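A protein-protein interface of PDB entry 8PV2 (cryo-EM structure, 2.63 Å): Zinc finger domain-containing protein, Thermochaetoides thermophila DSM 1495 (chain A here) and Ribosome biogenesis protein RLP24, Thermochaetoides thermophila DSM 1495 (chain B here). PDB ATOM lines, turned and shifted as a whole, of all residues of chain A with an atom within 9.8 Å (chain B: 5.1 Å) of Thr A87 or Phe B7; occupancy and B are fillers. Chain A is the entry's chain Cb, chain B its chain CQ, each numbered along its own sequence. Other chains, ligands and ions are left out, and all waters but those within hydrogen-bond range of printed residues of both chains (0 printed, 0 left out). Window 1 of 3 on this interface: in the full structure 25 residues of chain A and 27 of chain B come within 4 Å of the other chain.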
ATOM      1  N   ASP A  18      16.419  12.454  20.819  1.00  0.00           N
ATOM      2  CA  ASP A  18      16.094  13.101  19.559  1.00  0.00           C
ATOM      3  C   ASP A  18      17.331  13.349  18.705  1.00  0.00           C
ATOM      4  O   ASP A  18      18.469  13.338  19.185  1.00  0.00           O
ATOM      5  CB  ASP A  18      15.367  14.420  19.803  1.00  0.00           C
ATOM      6  CG  ASP A  18      13.950  14.221  20.290  1.00  0.00           C
ATOM      7  OD1 ASP A  18      13.320  13.220  19.892  1.00  0.00           O
ATOM      8  OD2 ASP A  18      13.458  15.063  21.070  1.00  0.00           O
ATOM      9  N   LEU A  19      17.081  13.601  17.418  1.00  0.00           N
ATOM     10  CA  LEU A  19      18.158  13.709  16.441  1.00  0.00           C
ATOM     11  C   LEU A  19      18.960  14.990  16.624  1.00  0.00           C
ATOM     12  O   LEU A  19      20.160  15.021  16.334  1.00  0.00           O
ATOM     13  CB  LEU A  19      17.580  13.631  15.030  1.00  0.00           C
ATOM     14  CG  LEU A  19      18.547  13.291  13.899  1.00  0.00           C
ATOM     15  CD1 LEU A  19      19.053  11.867  14.029  1.00  0.00           C
ATOM     16  CD2 LEU A  19      17.880  13.509  12.562  1.00  0.00           C
ATOM     17  N   ASP A  20      18.318  16.065  17.088  1.00  0.00           N
ATOM     18  CA  ASP A  20      19.062  17.294  17.356  1.00  0.00           C
ATOM     19  C   ASP A  20      20.006  17.118  18.537  1.00  0.00           C
ATOM     20  O   ASP A  20      21.138  17.619  18.519  1.00  0.00           O
ATOM     21  CB  ASP A  20      18.097  18.455  17.592  1.00  0.00           C
ATOM     22  CG  ASP A  20      16.937  18.085  18.491  1.00  0.00           C
ATOM     23  OD1 ASP A  20      17.162  17.491  19.563  1.00  0.00           O
ATOM     24  OD2 ASP A  20      15.786  18.394  18.123  1.00  0.00           O
ATOM     25  N   GLN A  21      19.561  16.396  19.566  1.00  0.00           N
ATOM     26  CA  GLN A  21      20.450  16.044  20.665  1.00  0.00           C
ATOM     27  C   GLN A  21      21.572  15.129  20.192  1.00  0.00           C
ATOM     28  O   GLN A  21      22.701  15.222  20.684  1.00  0.00           O
ATOM     29  CB  GLN A  21      19.655  15.387  21.789  1.00  0.00           C
ATOM     30  CG  GLN A  21      18.553  16.259  22.338  1.00  0.00           C
ATOM     31  CD  GLN A  21      17.749  15.578  23.416  1.00  0.00           C
ATOM     32  OE1 GLN A  21      16.977  14.662  23.146  1.00  0.00           O
ATOM     33  NE2 GLN A  21      17.925  16.025  24.650  1.00  0.00           N
ATOM     34  N   ILE A  22      21.285  14.250  19.230  1.00  0.00           N
ATOM     35  CA  ILE A  22      22.327  13.400  18.657  1.00  0.00           C
ATOM     36  C   ILE A  22      23.361  14.237  17.904  1.00  0.00           C
ATOM     37  O   ILE A  22      24.568  13.986  17.998  1.00  0.00           O
ATOM     38  CB  ILE A  22      21.686  12.317  17.767  1.00  0.00           C
ATOM     39  CG1 ILE A  22      20.966  11.290  18.644  1.00  0.00           C
ATOM     40  CG2 ILE A  22      22.712  11.626  16.889  1.00  0.00           C
ATOM     41  CD1 ILE A  22      20.048  10.369  17.888  1.00  0.00           C
ATOM     42  N   GLU A  23      22.909  15.252  17.162  1.00  0.00           N
ATOM     43  CA  GLU A  23      23.837  16.160  16.488  1.00  0.00           C
ATOM     44  C   GLU A  23      24.698  16.932  17.479  1.00  0.00           C
ATOM     45  O   GLU A  23      25.901  17.121  17.257  1.00  0.00           O
ATOM     46  CB  GLU A  23      23.085  17.131  15.580  1.00  0.00           C
ATOM     47  CG  GLU A  23      22.883  16.622  14.177  1.00  0.00           C
ATOM     48  CD  GLU A  23      22.112  17.585  13.306  1.00  0.00           C
ATOM     49  OE1 GLU A  23      22.397  18.798  13.363  1.00  0.00           O
ATOM     50  OE2 GLU A  23      21.268  17.124  12.515  1.00  0.00           O
ATOM     51  N   ARG A  24      24.096  17.399  18.575  1.00  0.00           N
ATOM     52  CA  ARG A  24      24.877  18.082  19.603  1.00  0.00           C
ATOM     53  C   ARG A  24      25.891  17.146  20.249  1.00  0.00           C
ATOM     54  O   ARG A  24      27.020  17.553  20.547  1.00  0.00           O
ATOM     55  CB  ARG A  24      23.950  18.685  20.656  1.00  0.00           C
ATOM     56  CG  ARG A  24      23.012  19.750  20.117  1.00  0.00           C
ATOM     57  CD  ARG A  24      22.972  20.958  21.032  1.00  0.00           C
ATOM     58  NE  ARG A  24      24.261  21.636  21.097  1.00  0.00           N
ATOM     59  CZ  ARG A  24      24.789  22.132  22.207  1.00  0.00           C
ATOM     60  NH1 ARG A  24      24.166  22.042  23.370  1.00  0.00           N
ATOM     61  NH2 ARG A  24      25.974  22.733  22.149  1.00  0.00           N
ATOM     62  N   ARG A  27      28.788  16.761  17.747  1.00  0.00           N
ATOM     63  CA  ARG A  27      29.665  17.912  17.569  1.00  0.00           C
ATOM     64  C   ARG A  27      30.424  18.260  18.846  1.00  0.00           C
ATOM     65  O   ARG A  27      31.527  18.810  18.774  1.00  0.00           O
ATOM     66  CB  ARG A  27      28.874  19.122  17.074  1.00  0.00           C
ATOM     67  CG  ARG A  27      27.886  19.694  18.067  1.00  0.00           C
ATOM     68  CD  ARG A  27      27.085  20.813  17.444  1.00  0.00           C
ATOM     69  NE  ARG A  27      26.192  20.309  16.410  1.00  0.00           N
ATOM     70  CZ  ARG A  27      25.480  21.076  15.599  1.00  0.00           C
ATOM     71  NH1 ARG A  27      25.520  22.395  15.686  1.00  0.00           N
ATOM     72  NH2 ARG A  27      24.710  20.507  14.677  1.00  0.00           N
ATOM     73  N   GLU A  83      21.140  14.588   6.275  1.00  0.00           N
ATOM     74  CA  GLU A  83      20.153  15.598   5.906  1.00  0.00           C
ATOM     75  C   GLU A  83      20.096  16.732   6.922  1.00  0.00           C
ATOM     76  O   GLU A  83      19.916  17.892   6.542  1.00  0.00           O
ATOM     77  CB  GLU A  83      18.780  14.954   5.753  1.00  0.00           C
ATOM     78  CG  GLU A  83      18.689  13.996   4.585  1.00  0.00           C
ATOM     79  CD  GLU A  83      17.325  13.352   4.466  1.00  0.00           C
ATOM     80  OE1 GLU A  83      16.489  13.557   5.370  1.00  0.00           O
ATOM     81  OE2 GLU A  83      17.093  12.631   3.474  1.00  0.00           O
ATOM     82  N   GLY A  84      20.254  16.423   8.205  1.00  0.00           N
ATOM     83  CA  GLY A  84      20.233  17.438   9.240  1.00  0.00           C
ATOM     84  C   GLY A  84      18.970  17.393  10.070  1.00  0.00           C
ATOM     85  O   GLY A  84      17.873  17.250   9.523  1.00  0.00           O
ATOM     86  N   ALA A  85      19.103  17.499  11.389  1.00  0.00           N
ATOM     87  CA  ALA A  85      17.932  17.467  12.251  1.00  0.00           C
ATOM     88  C   ALA A  85      17.173  18.781  12.178  1.00  0.00           C
ATOM     89  O   ALA A  85      17.723  19.829  11.835  1.00  0.00           O
ATOM     90  CB  ALA A  85      18.316  17.181  13.700  1.00  0.00           C
ATOM     91  N   TYR A  86      15.890  18.711  12.504  1.00  0.00           N
ATOM     92  CA  TYR A  86      15.056  19.897  12.549  1.00  0.00           C
ATOM     93  C   TYR A  86      15.238  20.602  13.883  1.00  0.00           C
ATOM     94  O   TYR A  86      15.202  19.974  14.943  1.00  0.00           O
ATOM     95  CB  TYR A  86      13.597  19.517  12.342  1.00  0.00           C
ATOM     96  CG  TYR A  86      12.684  20.686  12.128  1.00  0.00           C
ATOM     97  CD1 TYR A  86      12.738  21.413  10.953  1.00  0.00           C
ATOM     98  CD2 TYR A  86      11.745  21.043  13.080  1.00  0.00           C
ATOM     99  CE1 TYR A  86      11.902  22.473  10.742  1.00  0.00           C
ATOM    100  CE2 TYR A  86      10.899  22.101  12.870  1.00  0.00           C
ATOM    101  CZ  TYR A  86      10.983  22.811  11.700  1.00  0.00           C
ATOM    102  OH  TYR A  86      10.137  23.865  11.482  1.00  0.00           O
ATOM    103  N   THR A  87      15.452  21.914  13.827  1.00  0.00           N
ATOM    104  CA  THR A  87      15.795  22.701  15.002  1.00  0.00           C
ATOM    105  C   THR A  87      15.005  24.007  15.003  1.00  0.00           C
ATOM    106  O   THR A  87      14.269  24.325  14.061  1.00  0.00           O
ATOM    107  CB  THR A  87      17.302  22.979  15.064  1.00  0.00           C
ATOM    108  OG1 THR A  87      17.757  23.460  13.793  1.00  0.00           O
ATOM    109  CG2 THR A  87      18.090  21.721  15.467  1.00  0.00           C
ATOM    110  N   HIS A  88      15.178  24.774  16.083  1.00  0.00           N
ATOM    111  CA  HIS A  88      14.412  26.002  16.262  1.00  0.00           C
ATOM    112  C   HIS A  88      14.822  27.092  15.282  1.00  0.00           C
ATOM    113  O   HIS A  88      13.977  27.888  14.869  1.00  0.00           O
ATOM    114  CB  HIS A  88      14.552  26.506  17.694  1.00  0.00           C
ATOM    115  CG  HIS A  88      13.618  25.847  18.657  1.00  0.00           C
ATOM    116  ND1 HIS A  88      13.950  24.701  19.345  1.00  0.00           N
ATOM    117  CD2 HIS A  88      12.366  26.173  19.052  1.00  0.00           C
ATOM    118  CE1 HIS A  88      12.943  24.350  20.123  1.00  0.00           C
ATOM    119  NE2 HIS A  88      11.968  25.226  19.964  1.00  0.00           N
ATOM    120  N   GLU A  89      16.100  27.158  14.899  1.00  0.00           N
ATOM    121  CA  GLU A  89      16.502  28.176  13.933  1.00  0.00           C
ATOM    122  C   GLU A  89      15.969  27.866  12.537  1.00  0.00           C
ATOM    123  O   GLU A  89      15.593  28.783  11.797  1.00  0.00           O
ATOM    124  CB  GLU A  89      18.023  28.357  13.939  1.00  0.00           C
ATOM    125  CG  GLU A  89      18.852  27.209  13.402  1.00  0.00           C
ATOM    126  CD  GLU A  89      19.141  26.141  14.447  1.00  0.00           C
ATOM    127  OE1 GLU A  89      18.473  26.116  15.503  1.00  0.00           O
ATOM    128  OE2 GLU A  89      20.053  25.322  14.208  1.00  0.00           O
ATOM    129  N   GLU A  90      15.898  26.584  12.166  1.00  0.00           N
ATOM    130  CA  GLU A  90      15.249  26.228  10.910  1.00  0.00           C
ATOM    131  C   GLU A  90      13.754  26.507  10.971  1.00  0.00           C
ATOM    132  O   GLU A  90      13.160  26.963   9.986  1.00  0.00           O
ATOM    133  CB  GLU A  90      15.502  24.760  10.573  1.00  0.00           C
ATOM    134  CG  GLU A  90      14.916  24.356   9.230  1.00  0.00           C
ATOM    135  CD  GLU A  90      15.196  22.920   8.856  1.00  0.00           C
ATOM    136  OE1 GLU A  90      15.838  22.211   9.656  1.00  0.00           O
ATOM    137  OE2 GLU A  90      14.774  22.500   7.760  1.00  0.00           O
ATOM    138  N   ALA A  91      13.137  26.259  12.130  1.00  0.00           N
ATOM    139  CA  ALA A  91      11.721  26.575  12.308  1.00  0.00           C
ATOM    140  C   ALA A  91      11.465  28.070  12.184  1.00  0.00           C
ATOM    141  O   ALA A  91      10.437  28.493  11.646  1.00  0.00           O
ATOM    142  CB  ALA A  91      11.241  26.062  13.664  1.00  0.00           C
ATOM    143  N   MET A  92      12.391  28.881  12.688  1.00  0.00           N
ATOM    144  CA  MET A  92      12.260  30.328  12.607  1.00  0.00           C
ATOM    145  C   MET A  92      12.470  30.823  11.176  1.00  0.00           C
ATOM    146  O   MET A  92      11.745  31.707  10.694  1.00  0.00           O
ATOM    147  CB  MET A  92      13.258  30.949  13.579  1.00  0.00           C
ATOM    148  CG  MET A  92      13.189  32.427  13.728  1.00  0.00           C
ATOM    149  SD  MET A  92      14.397  33.045  14.907  1.00  0.00           S
ATOM    150  CE  MET A  92      13.672  32.471  16.434  1.00  0.00           C
ATOM    151  N   ALA A  93      13.440  30.243  10.470  1.00  0.00           N
ATOM    152  CA  ALA A  93      13.667  30.615   9.078  1.00  0.00           C
ATOM    153  C   ALA A  93      12.518  30.176   8.178  1.00  0.00           C
ATOM    154  O   ALA A  93      12.295  30.787   7.128  1.00  0.00           O
ATOM    155  CB  ALA A  93      14.981  30.018   8.586  1.00  0.00           C
ATOM    156  N   ALA A  94      11.791  29.123   8.570  1.00  0.00           N
ATOM    157  CA  ALA A  94      10.666  28.639   7.773  1.00  0.00           C
ATOM    158  C   ALA A  94       9.543  29.660   7.685  1.00  0.00           C
ATOM    159  O   ALA A  94       8.822  29.700   6.683  1.00  0.00           O
ATOM    160  CB  ALA A  94      10.140  27.333   8.357  1.00  0.00           C
ATOM    161  N   ILE A  95       9.370  30.480   8.717  1.00  0.00           N
ATOM    162  CA  ILE A  95       8.407  31.569   8.687  1.00  0.00           C
ATOM    163  C   ILE A  95       9.080  32.903   8.413  1.00  0.00           C
ATOM    164  O   ILE A  95       8.399  33.928   8.315  1.00  0.00           O
ATOM    165  CB  ILE A  95       7.583  31.630   9.983  1.00  0.00           C
ATOM    166  CG1 ILE A  95       8.511  31.658  11.193  1.00  0.00           C
ATOM    167  CG2 ILE A  95       6.606  30.470  10.051  1.00  0.00           C
ATOM    168  CD1 ILE A  95       7.799  31.722  12.501  1.00  0.00           C
ATOM    169  N   ASN B   5       4.549  30.787  17.347  1.00  0.00           N
ATOM    170  CA  ASN B   5       4.412  29.974  16.152  1.00  0.00           C
ATOM    171  C   ASN B   5       4.673  28.523  16.505  1.00  0.00           C
ATOM    172  O   ASN B   5       5.445  28.220  17.417  1.00  0.00           O
ATOM    173  CB  ASN B   5       5.352  30.433  15.042  1.00  0.00           C
ATOM    174  CG  ASN B   5       4.796  31.604  14.268  1.00  0.00           C
ATOM    175  OD1 ASN B   5       4.135  31.430  13.245  1.00  0.00           O
ATOM    176  ND2 ASN B   5       5.054  32.807  14.754  1.00  0.00           N
ATOM    177  N   CYS B   6       3.998  27.630  15.788  1.00  0.00           N
ATOM    178  CA  CYS B   6       4.179  26.206  16.012  1.00  0.00           C
ATOM    179  C   CYS B   6       5.585  25.795  15.606  1.00  0.00           C
ATOM    180  O   CYS B   6       6.079  26.188  14.547  1.00  0.00           O
ATOM    181  CB  CYS B   6       3.144  25.408  15.224  1.00  0.00           C
ATOM    182  SG  CYS B   6       3.200  23.624  15.494  1.00  0.00           S
ATOM    183  N   PHE B   7       6.235  25.018  16.472  1.00  0.00           N
ATOM    184  CA  PHE B   7       7.556  24.490  16.154  1.00  0.00           C
ATOM    185  C   PHE B   7       7.502  23.576  14.942  1.00  0.00           C
ATOM    186  O   PHE B   7       8.363  23.648  14.061  1.00  0.00           O
ATOM    187  CB  PHE B   7       8.119  23.743  17.362  1.00  0.00           C
ATOM    188  CG  PHE B   7       9.370  22.961  17.075  1.00  0.00           C
ATOM    189  CD1 PHE B   7      10.595  23.596  16.985  1.00  0.00           C
ATOM    190  CD2 PHE B   7       9.321  21.584  16.915  1.00  0.00           C
ATOM    191  CE1 PHE B   7      11.741  22.882  16.727  1.00  0.00           C
ATOM    192  CE2 PHE B   7      10.463  20.870  16.658  1.00  0.00           C
ATOM    193  CZ  PHE B   7      11.675  21.518  16.565  1.00  0.00           C
ATOM    194  N   PHE B   8       6.476  22.734  14.871  1.00  0.00           N
ATOM    195  CA  PHE B   8       6.428  21.692  13.858  1.00  0.00           C
ATOM    196  C   PHE B   8       5.989  22.240  12.505  1.00  0.00           C
ATOM    197  O   PHE B   8       6.716  22.117  11.514  1.00  0.00           O
ATOM    198  CB  PHE B   8       5.500  20.577  14.328  1.00  0.00           C
ATOM    199  CG  PHE B   8       5.812  19.242  13.742  1.00  0.00           C
ATOM    200  CD1 PHE B   8       5.171  18.807  12.601  1.00  0.00           C
ATOM    201  CD2 PHE B   8       6.742  18.414  14.339  1.00  0.00           C
ATOM    202  CE1 PHE B   8       5.457  17.576  12.066  1.00  0.00           C
ATOM    203  CE2 PHE B   8       7.030  17.179  13.807  1.00  0.00           C
ATOM    204  CZ  PHE B   8       6.394  16.766  12.666  1.00  0.00           C
ATOM    205  N   CYS B   9       4.815  22.863  12.445  1.00  0.00           N
ATOM    206  CA  CYS B   9       4.229  23.266  11.177  1.00  0.00           C
ATOM    207  C   CYS B   9       4.360  24.751  10.868  1.00  0.00           C
ATOM    208  O   CYS B   9       4.342  25.117   9.691  1.00  0.00           O
ATOM    209  CB  CYS B   9       2.748  22.869  11.133  1.00  0.00           C
ATOM    210  SG  CYS B   9       1.631  23.954  12.036  1.00  0.00           S
ATOM    211  N   GLY B  10       4.484  25.612  11.875  1.00  0.00           N
ATOM    212  CA  GLY B  10       4.674  27.028  11.654  1.00  0.00           C
ATOM    213  C   GLY B  10       3.427  27.883  11.717  1.00  0.00           C
ATOM    214  O   GLY B  10       3.516  29.088  11.461  1.00  0.00           O
ATOM    215  N   PHE B  29       9.210  23.293  23.251  1.00  0.00           N
ATOM    216  CA  PHE B  29       8.632  23.083  21.927  1.00  0.00           C
ATOM    217  C   PHE B  29       7.139  23.368  21.996  1.00  0.00           C
ATOM    218  O   PHE B  29       6.390  22.588  22.586  1.00  0.00           O
ATOM    219  CB  PHE B  29       8.874  21.654  21.442  1.00  0.00           C
ATOM    220  CG  PHE B  29      10.316  21.268  21.368  1.00  0.00           C
ATOM    221  CD1 PHE B  29      10.973  20.754  22.474  1.00  0.00           C
ATOM    222  CD2 PHE B  29      11.014  21.388  20.183  1.00  0.00           C
ATOM    223  CE1 PHE B  29      12.296  20.392  22.396  1.00  0.00           C
ATOM    224  CE2 PHE B  29      12.330  21.026  20.103  1.00  0.00           C
ATOM    225  CZ  PHE B  29      12.972  20.530  21.210  1.00  0.00           C
ATOM    226  N   ARG B  30       6.701  24.460  21.384  1.00  0.00           N
ATOM    227  CA  ARG B  30       5.289  24.811  21.365  1.00  0.00           C
ATOM    228  C   ARG B  30       4.638  24.289  20.092  1.00  0.00           C
ATOM    229  O   ARG B  30       5.089  24.595  18.987  1.00  0.00           O
ATOM    230  CB  ARG B  30       5.106  26.323  21.468  1.00  0.00           C
ATOM    231  CG  ARG B  30       3.693  26.807  21.212  1.00  0.00           C
ATOM    232  CD  ARG B  30       2.751  26.433  22.338  1.00  0.00           C
ATOM    233  NE  ARG B  30       1.406  26.938  22.101  1.00  0.00           N
ATOM    234  CZ  ARG B  30       1.009  28.176  22.364  1.00  0.00           C
ATOM    235  NH1 ARG B  30       1.828  29.069  22.890  1.00  0.00           N
ATOM    236  NH2 ARG B  30      -0.241  28.527  22.088  1.00  0.00           N
ATOM    237  N   PHE B  31       3.575  23.508  20.253  1.00  0.00           N
ATOM    238  CA  PHE B  31       2.796  22.979  19.151  1.00  0.00           C
ATOM    239  C   PHE B  31       1.414  23.601  19.176  1.00  0.00           C
ATOM    240  O   PHE B  31       0.822  23.790  20.241  1.00  0.00           O
ATOM    241  CB  PHE B  31       2.676  21.456  19.231  1.00  0.00           C
ATOM    242  CG  PHE B  31       3.979  20.767  19.441  1.00  0.00           C
ATOM    243  CD1 PHE B  31       4.888  20.665  18.408  1.00  0.00           C
ATOM    244  CD2 PHE B  31       4.307  20.241  20.675  1.00  0.00           C
ATOM    245  CE1 PHE B  31       6.092  20.050  18.601  1.00  0.00           C
ATOM    246  CE2 PHE B  31       5.512  19.626  20.870  1.00  0.00           C
ATOM    247  CZ  PHE B  31       6.403  19.532  19.835  1.00  0.00           C
ATOM    248  N   PHE B  40       5.392  14.923  16.185  1.00  0.00           N
ATOM    249  CA  PHE B  40       6.641  15.123  16.909  1.00  0.00           C
ATOM    250  C   PHE B  40       6.962  13.940  17.815  1.00  0.00           C
ATOM    251  O   PHE B  40       8.118  13.512  17.896  1.00  0.00           O
ATOM    252  CB  PHE B  40       6.556  16.419  17.712  1.00  0.00           C
ATOM    253  CG  PHE B  40       7.812  16.774  18.445  1.00  0.00           C
ATOM    254  CD1 PHE B  40       8.828  17.456  17.806  1.00  0.00           C
ATOM    255  CD2 PHE B  40       7.965  16.458  19.785  1.00  0.00           C
ATOM    256  CE1 PHE B  40       9.977  17.795  18.480  1.00  0.00           C
ATOM    257  CE2 PHE B  40       9.109  16.795  20.461  1.00  0.00           C
ATOM    258  CZ  PHE B  40      10.119  17.461  19.806  1.00  0.00           C
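O of Phe B7 is in hydrogen-bond range of OH of Tyr A86, at 3.1 Å.
Hydrophobic or aromatic side chains of chain B within 4 Å of the printed part of chain A: Phe B7 and Phe B29. Hydrophobic or aromatic side chains of chain A within 4 Å of the printed part of chain B: Tyr A86, His A88, Ala A91 and Ile A95. Among the printed residues, no Asp or Glu carboxylate lies within 4 Å of a Lys or Arg side-chain nitrogen of the other chain.
Among the printed residues, pairs that only touch across the chains: Tyr A86 with Phe B8 (3.8 Å), Thr A87 with Phe B7 (3.9 Å), His A88 with Phe B7 (3.7 Å), His A88 with Phe B29 (3.4 Å), Ala A91 with Phe B7 (3.8 Å), Ile A95 with Asn B5 (3.5 Å) and Ile A95 with Gly B10 (3.7 Å).
The backbone NH (N) of Phe B8 sits close to the side-chain sulfur (SG) of Cys B6 (3.5 Å). The backbone carbonyl oxygen (O) of Gly B10 sits close to the side-chain amide oxygen (OD1) of Asn B5. N of Phe B7 sits at hydrogen-bond distance from O of Arg B30 (2.8 Å). The side-chain carboxylate of Glu A89 is in hydrogen-bond range of the side-chain hydroxyl of Thr A87, 3.0 Å away.
Printed residues of chain B within 4 Å of Thr A87: Phe B7 (3.9 Å). No residue of chain A comes within 4 Å of Cys B6. Of the printed residues of chain A, Phe B8 touches Tyr A86. Cys B9 touches none of the printed residues of chain A. Printed residues of chain A within 4 Å of Phe B29: His A88 (3.4 Å). The nearest printed residue of chain B that does not touch Thr A87 is Phe B29 (6.4 Å).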
